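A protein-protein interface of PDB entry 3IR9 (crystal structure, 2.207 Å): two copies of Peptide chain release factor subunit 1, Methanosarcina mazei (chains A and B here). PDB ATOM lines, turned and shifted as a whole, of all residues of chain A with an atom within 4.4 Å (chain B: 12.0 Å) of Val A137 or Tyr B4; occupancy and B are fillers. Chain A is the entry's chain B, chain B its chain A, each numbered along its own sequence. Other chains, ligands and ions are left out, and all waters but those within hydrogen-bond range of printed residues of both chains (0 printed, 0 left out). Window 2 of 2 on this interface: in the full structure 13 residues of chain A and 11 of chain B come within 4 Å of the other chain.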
ATOM      1  N   GLY A  28      13.517   7.998   9.174  1.00  0.00           N
ATOM      2  CA  GLY A  28      13.647   7.030   8.099  1.00  0.00           C
ATOM      3  C   GLY A  28      13.688   7.680   6.728  1.00  0.00           C
ATOM      4  O   GLY A  28      14.472   7.277   5.871  1.00  0.00           O
ATOM      5  N   GLN A  29      12.842   8.685   6.521  1.00  0.00           N
ATOM      6  CA  GLN A  29      12.812   9.409   5.260  1.00  0.00           C
ATOM      7  C   GLN A  29      14.111  10.167   5.048  1.00  0.00           C
ATOM      8  O   GLN A  29      14.481  10.465   3.915  1.00  0.00           O
ATOM      9  CB  GLN A  29      11.637  10.379   5.223  1.00  0.00           C
ATOM     10  CG  GLN A  29      10.287   9.713   5.320  1.00  0.00           C
ATOM     11  CD  GLN A  29       9.176  10.729   5.435  1.00  0.00           C
ATOM     12  OE1 GLN A  29       9.376  11.911   5.144  1.00  0.00           O
ATOM     13  NE2 GLN A  29       7.999  10.279   5.866  1.00  0.00           N
ATOM     14  N   ASN A  31      16.895   8.786   6.352  1.00  0.00           N
ATOM     15  CA  ASN A  31      17.713   7.629   6.019  1.00  0.00           C
ATOM     16  C   ASN A  31      17.782   7.446   4.511  1.00  0.00           C
ATOM     17  O   ASN A  31      18.858   7.295   3.941  1.00  0.00           O
ATOM     18  CB  ASN A  31      17.145   6.361   6.654  1.00  0.00           C
ATOM     19  CG  ASN A  31      17.320   6.336   8.153  1.00  0.00           C
ATOM     20  OD1 ASN A  31      18.140   7.071   8.702  1.00  0.00           O
ATOM     21  ND2 ASN A  31      16.549   5.487   8.829  1.00  0.00           N
ATOM     22  N   ALA A  32      16.619   7.481   3.870  1.00  0.00           N
ATOM     23  CA  ALA A  32      16.494   7.156   2.451  1.00  0.00           C
ATOM     24  C   ALA A  32      17.067   8.218   1.515  1.00  0.00           C
ATOM     25  O   ALA A  32      17.701   7.887   0.510  1.00  0.00           O
ATOM     26  CB  ALA A  32      15.042   6.878   2.106  1.00  0.00           C
ATOM     27  N   ASP A  35      20.856   8.126   1.771  1.00  0.00           N
ATOM     28  CA  ASP A  35      21.384   6.963   1.067  1.00  0.00           C
ATOM     29  C   ASP A  35      21.360   7.157  -0.448  1.00  0.00           C
ATOM     30  O   ASP A  35      22.257   6.689  -1.150  1.00  0.00           O
ATOM     31  CB  ASP A  35      20.623   5.697   1.469  1.00  0.00           C
ATOM     32  CG  ASP A  35      20.829   5.330   2.931  1.00  0.00           C
ATOM     33  OD1 ASP A  35      21.486   6.109   3.657  1.00  0.00           O
ATOM     34  OD2 ASP A  35      20.336   4.262   3.351  1.00  0.00           O
ATOM     35  N   VAL A  65      15.205   1.038  -4.267  1.00  0.00           N
ATOM     36  CA  VAL A  65      14.427   1.955  -3.430  1.00  0.00           C
ATOM     37  C   VAL A  65      13.984   3.184  -4.225  1.00  0.00           C
ATOM     38  O   VAL A  65      14.788   3.800  -4.925  1.00  0.00           O
ATOM     39  CB  VAL A  65      15.238   2.422  -2.195  1.00  0.00           C
ATOM     40  CG1 VAL A  65      14.591   3.633  -1.550  1.00  0.00           C
ATOM     41  CG2 VAL A  65      15.375   1.292  -1.185  1.00  0.00           C
ATOM     42  N   LEU A  66      12.706   3.539  -4.109  1.00  0.00           N
ATOM     43  CA  LEU A  66      12.143   4.658  -4.869  1.00  0.00           C
ATOM     44  C   LEU A  66      11.687   5.817  -3.985  1.00  0.00           C
ATOM     45  O   LEU A  66      10.987   5.617  -2.993  1.00  0.00           O
ATOM     46  CB  LEU A  66      10.979   4.188  -5.749  1.00  0.00           C
ATOM     47  CG  LEU A  66      10.107   5.277  -6.385  1.00  0.00           C
ATOM     48  CD1 LEU A  66      10.901   6.121  -7.374  1.00  0.00           C
ATOM     49  CD2 LEU A  66       8.881   4.668  -7.054  1.00  0.00           C
ATOM     50  N   LEU A  67      12.080   7.029  -4.367  1.00  0.00           N
ATOM     51  CA  LEU A  67      11.796   8.228  -3.582  1.00  0.00           C
ATOM     52  C   LEU A  67      10.787   9.144  -4.276  1.00  0.00           C
ATOM     53  O   LEU A  67      11.023   9.606  -5.396  1.00  0.00           O
ATOM     54  CB  LEU A  67      13.091   8.999  -3.306  1.00  0.00           C
ATOM     55  CG  LEU A  67      13.977   8.496  -2.160  1.00  0.00           C
ATOM     56  CD1 LEU A  67      14.337   7.032  -2.325  1.00  0.00           C
ATOM     57  CD2 LEU A  67      15.236   9.341  -2.072  1.00  0.00           C
ATOM     58  N   LEU A  68       9.670   9.408  -3.601  1.00  0.00           N
ATOM     59  CA  LEU A  68       8.617  10.263  -4.150  1.00  0.00           C
ATOM     60  C   LEU A  68       8.276  11.424  -3.215  1.00  0.00           C
ATOM     61  O   LEU A  68       7.910  11.208  -2.062  1.00  0.00           O
ATOM     62  CB  LEU A  68       7.354   9.444  -4.429  1.00  0.00           C
ATOM     63  CG  LEU A  68       7.422   8.252  -5.393  1.00  0.00           C
ATOM     64  CD1 LEU A  68       6.128   7.463  -5.336  1.00  0.00           C
ATOM     65  CD2 LEU A  68       7.708   8.680  -6.829  1.00  0.00           C
ATOM     66  N   LYS A 135      11.161  -0.837  -2.558  1.00  0.00           N
ATOM     67  CA  LYS A 135      10.756  -0.152  -1.334  1.00  0.00           C
ATOM     68  C   LYS A 135      10.404   1.312  -1.631  1.00  0.00           C
ATOM     69  O   LYS A 135      11.244   2.073  -2.110  1.00  0.00           O
ATOM     70  CB  LYS A 135      11.858  -0.263  -0.266  1.00  0.00           C
ATOM     71  CG  LYS A 135      12.389  -1.691  -0.057  1.00  0.00           C
ATOM     72  CD  LYS A 135      13.228  -1.837   1.222  1.00  0.00           C
ATOM     73  CE  LYS A 135      14.696  -1.465   1.012  1.00  0.00           C
ATOM     74  NZ  LYS A 135      15.464  -2.486   0.233  1.00  0.00           N
ATOM     75  N   VAL A 136       9.159   1.698  -1.355  1.00  0.00           N
ATOM     76  CA  VAL A 136       8.681   3.045  -1.682  1.00  0.00           C
ATOM     77  C   VAL A 136       8.665   4.000  -0.483  1.00  0.00           C
ATOM     78  O   VAL A 136       8.072   3.699   0.551  1.00  0.00           O
ATOM     79  CB  VAL A 136       7.268   3.021  -2.294  1.00  0.00           C
ATOM     80  CG1 VAL A 136       6.858   4.428  -2.704  1.00  0.00           C
ATOM     81  CG2 VAL A 136       7.209   2.066  -3.484  1.00  0.00           C
ATOM     82  N   VAL A 137       9.303   5.159  -0.642  1.00  0.00           N
ATOM     83  CA  VAL A 137       9.400   6.150   0.431  1.00  0.00           C
ATOM     84  C   VAL A 137       8.978   7.556  -0.026  1.00  0.00           C
ATOM     85  O   VAL A 137       9.464   8.056  -1.039  1.00  0.00           O
ATOM     86  CB  VAL A 137      10.834   6.210   0.997  1.00  0.00           C
ATOM     87  CG1 VAL A 137      10.888   7.130   2.210  1.00  0.00           C
ATOM     88  CG2 VAL A 137      11.339   4.803   1.344  1.00  0.00           C
ATOM     89  N   PHE A 138       8.075   8.189   0.725  1.00  0.00           N
ATOM     90  CA  PHE A 138       7.616   9.547   0.410  1.00  0.00           C
ATOM     91  C   PHE A 138       8.364  10.616   1.199  1.00  0.00           C
ATOM     92  O   PHE A 138       8.372  10.594   2.427  1.00  0.00           O
ATOM     93  CB  PHE A 138       6.118   9.678   0.668  1.00  0.00           C
ATOM     94  CG  PHE A 138       5.271   9.023  -0.374  1.00  0.00           C
ATOM     95  CD1 PHE A 138       4.668   9.776  -1.367  1.00  0.00           C
ATOM     96  CD2 PHE A 138       5.084   7.652  -0.370  1.00  0.00           C
ATOM     97  CE1 PHE A 138       3.885   9.174  -2.334  1.00  0.00           C
ATOM     98  CE2 PHE A 138       4.304   7.043  -1.334  1.00  0.00           C
ATOM     99  CZ  PHE A 138       3.703   7.806  -2.318  1.00  0.00           C
ATOM    100  N   VAL A 139       8.979  11.557   0.491  1.00  0.00           N
ATOM    101  CA  VAL A 139       9.826  12.558   1.131  1.00  0.00           C
ATOM    102  C   VAL A 139       9.240  13.966   1.008  1.00  0.00           C
ATOM    103  O   VAL A 139       8.678  14.329  -0.027  1.00  0.00           O
ATOM    104  CB  VAL A 139      11.257  12.514   0.556  1.00  0.00           C
ATOM    105  CG1 VAL A 139      12.151  13.492   1.284  1.00  0.00           C
ATOM    106  CG2 VAL A 139      11.821  11.108   0.666  1.00  0.00           C
ATOM    107  N   ALA B   3      13.125  -1.098   5.568  1.00  0.00           N
ATOM    108  CA  ALA B   3      14.449  -0.520   5.782  1.00  0.00           C
ATOM    109  C   ALA B   3      14.377   0.990   6.015  1.00  0.00           C
ATOM    110  O   ALA B   3      15.241   1.565   6.682  1.00  0.00           O
ATOM    111  CB  ALA B   3      15.375  -0.843   4.602  1.00  0.00           C
ATOM    112  N   TYR B   4      13.339   1.624   5.469  1.00  0.00           N
ATOM    113  CA  TYR B   4      13.179   3.078   5.567  1.00  0.00           C
ATOM    114  C   TYR B   4      11.791   3.525   6.060  1.00  0.00           C
ATOM    115  O   TYR B   4      11.541   4.721   6.244  1.00  0.00           O
ATOM    116  CB  TYR B   4      13.489   3.750   4.222  1.00  0.00           C
ATOM    117  CG  TYR B   4      14.837   3.396   3.633  1.00  0.00           C
ATOM    118  CD1 TYR B   4      15.981   4.097   3.995  1.00  0.00           C
ATOM    119  CD2 TYR B   4      14.964   2.367   2.706  1.00  0.00           C
ATOM    120  CE1 TYR B   4      17.215   3.780   3.453  1.00  0.00           C
ATOM    121  CE2 TYR B   4      16.192   2.042   2.162  1.00  0.00           C
ATOM    122  CZ  TYR B   4      17.315   2.752   2.537  1.00  0.00           C
ATOM    123  OH  TYR B   4      18.539   2.430   1.994  1.00  0.00           O
ATOM    124  N   THR B   5      10.890   2.571   6.264  1.00  0.00           N
ATOM    125  CA  THR B   5       9.556   2.878   6.777  1.00  0.00           C
ATOM    126  C   THR B   5       8.923   1.610   7.362  1.00  0.00           C
ATOM    127  O   THR B   5       9.264   0.497   6.948  1.00  0.00           O
ATOM    128  CB  THR B   5       8.660   3.539   5.691  1.00  0.00           C
ATOM    129  OG1 THR B   5       8.986   4.936   5.581  1.00  0.00           O
ATOM    130  CG2 THR B   5       7.179   3.393   6.023  1.00  0.00           C
ATOM    131  N   ASP B   6       8.028   1.779   8.335  1.00  0.00           N
ATOM    132  CA  ASP B   6       7.498   0.652   9.108  1.00  0.00           C
ATOM    133  C   ASP B   6       6.882  -0.450   8.252  1.00  0.00           C
ATOM    134  O   ASP B   6       6.285  -0.180   7.207  1.00  0.00           O
ATOM    135  CB  ASP B   6       6.474   1.123  10.138  1.00  0.00           C
ATOM    136  CG  ASP B   6       5.965  -0.010  11.007  1.00  0.00           C
ATOM    137  OD1 ASP B   6       4.740  -0.068  11.250  1.00  0.00           O
ATOM    138  OD2 ASP B   6       6.788  -0.852  11.433  1.00  0.00           O
ATOM    139  N   GLU B   7       7.020  -1.688   8.727  1.00  0.00           N
ATOM    140  CA  GLU B   7       6.593  -2.874   7.988  1.00  0.00           C
ATOM    141  C   GLU B   7       5.897  -3.876   8.915  1.00  0.00           C
ATOM    142  O   GLU B   7       5.024  -4.642   8.492  1.00  0.00           O
ATOM    143  CB  GLU B   7       7.812  -3.537   7.345  1.00  0.00           C
ATOM    144  CG  GLU B   7       7.626  -3.937   5.896  1.00  0.00           C
ATOM    145  CD  GLU B   7       7.791  -2.766   4.948  1.00  0.00           C
ATOM    146  OE1 GLU B   7       7.047  -1.773   5.091  1.00  0.00           O
ATOM    147  OE2 GLU B   7       8.664  -2.841   4.056  1.00  0.00           O
ATOM    148  N   SER B   8       6.303  -3.865  10.181  1.00  0.00           N
ATOM    149  CA  SER B   8       5.702  -4.710  11.203  1.00  0.00           C
ATOM    150  C   SER B   8       4.253  -4.304  11.422  1.00  0.00           C
ATOM    151  O   SER B   8       3.540  -4.917  12.215  1.00  0.00           O
ATOM    152  CB  SER B   8       6.469  -4.566  12.510  1.00  0.00           C
ATOM    153  OG  SER B   8       6.555  -3.199  12.872  1.00  0.00           O
ATOM    154  N   GLY B   9       3.836  -3.247  10.732  1.00  0.00           N
ATOM    155  CA  GLY B   9       2.455  -2.807  10.750  1.00  0.00           C
ATOM    156  C   GLY B   9       1.981  -2.229  12.067  1.00  0.00           C
ATOM    157  O   GLY B   9       0.839  -2.458  12.466  1.00  0.00           O
ATOM    158  N   SER B  11       2.593   1.155  12.471  1.00  0.00           N
ATOM    159  CA  SER B  11       2.132   2.375  11.834  1.00  0.00           C
ATOM    160  C   SER B  11       0.662   2.218  11.493  1.00  0.00           C
ATOM    161  O   SER B  11      -0.162   3.009  11.935  1.00  0.00           O
ATOM    162  CB  SER B  11       2.934   2.659  10.565  1.00  0.00           C
ATOM    163  OG  SER B  11       4.279   2.959  10.881  1.00  0.00           O
ATOM    164  N   GLU B  12       0.345   1.181  10.721  1.00  0.00           N
ATOM    165  CA  GLU B  12      -1.032   0.887  10.331  1.00  0.00           C
ATOM    166  C   GLU B  12      -1.959   0.718  11.540  1.00  0.00           C
ATOM    167  O   GLU B  12      -3.123   1.115  11.493  1.00  0.00           O
ATOM    168  CB  GLU B  12      -1.083  -0.367   9.453  1.00  0.00           C
ATOM    169  CG  GLU B  12      -0.251  -0.267   8.186  1.00  0.00           C
ATOM    170  CD  GLU B  12      -0.723   0.843   7.265  1.00  0.00           C
ATOM    171  OE1 GLU B  12       0.073   1.283   6.407  1.00  0.00           O
ATOM    172  OE2 GLU B  12      -1.889   1.275   7.398  1.00  0.00           O
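The side-chain hydroxyl (OH) of Tyr B4 is in hydrogen-bond range of the side-chain carboxylate (OD2) of Asp A35 (2.9 Å).
The backbone NH (N) of Leu A66 is in hydrogen-bond range of the backbone carbonyl oxygen (O) of Lys A135. O of Leu A66 is in hydrogen-bond range of N of Val A137 (2.9 Å). O of Val A137 lies within hydrogen-bond range of N of Leu A68 (2.9 Å).
Among the printed residues, pairs that only touch across the chains: Gly A28 with Tyr B4 (3.6 Å), Asn A31 with Tyr B4 (3.7 Å), Ala A32 with Tyr B4 (3.4 Å), Val A65 with Tyr B4 (3.5 Å), Lys A135 with Ala B3 (3.7 Å), Lys A135 with Tyr B4 (3.98 Å) and Val A137 with Tyr B4 (3.7 Å).
No residue of chain B comes within 4 Å of Gln A29. Asn A31 touches just one residue of chain B: Tyr B4. Ala A32 touches just one residue of chain B: Tyr B4 (3.4 Å). Asp A35 touches just one residue of chain B: Tyr B4 (2.9 Å). Val A65 touches just one residue of chain B: Tyr B4 (3.5 Å). Leu A66 touches none of the printed residues of chain B. No residue of chain B comes within 4 Å of Leu A68. Of the printed residues of chain B, Lys A135 touches Ala B3 (3.7 Å) and Tyr B4 (3.98 Å). No residue of chain B comes within 4 Å of Val A136. Val A137 touches one residue of chain B. No residue of chain B comes within 4 Å of Phe A138. No residue of chain B comes within 4 Å of Val A139. Of the printed residues of chain A, Ala B3 touches Lys A135 (3.7 Å). Of the printed residues of chain A, Tyr B4 touches Gly A28, Asn A31, Ala A32, Asp A35, Val A65, Lys A135 and Val A137. Glu B7 touches none of the printed residues of chain A. Ser B11 touches none of the printed residues of chain A.
Among the printed residues, 8 pairs touch across the chains. Among the printed residues, no Asp or Glu carboxylate lies within 4 Å of a Lys or Arg side-chain nitrogen of the other chain.
No position is printed for both chains. Of the 8 pairs that touch across the chains among the printed residues, none has its exchanged pair printed and touching as well.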
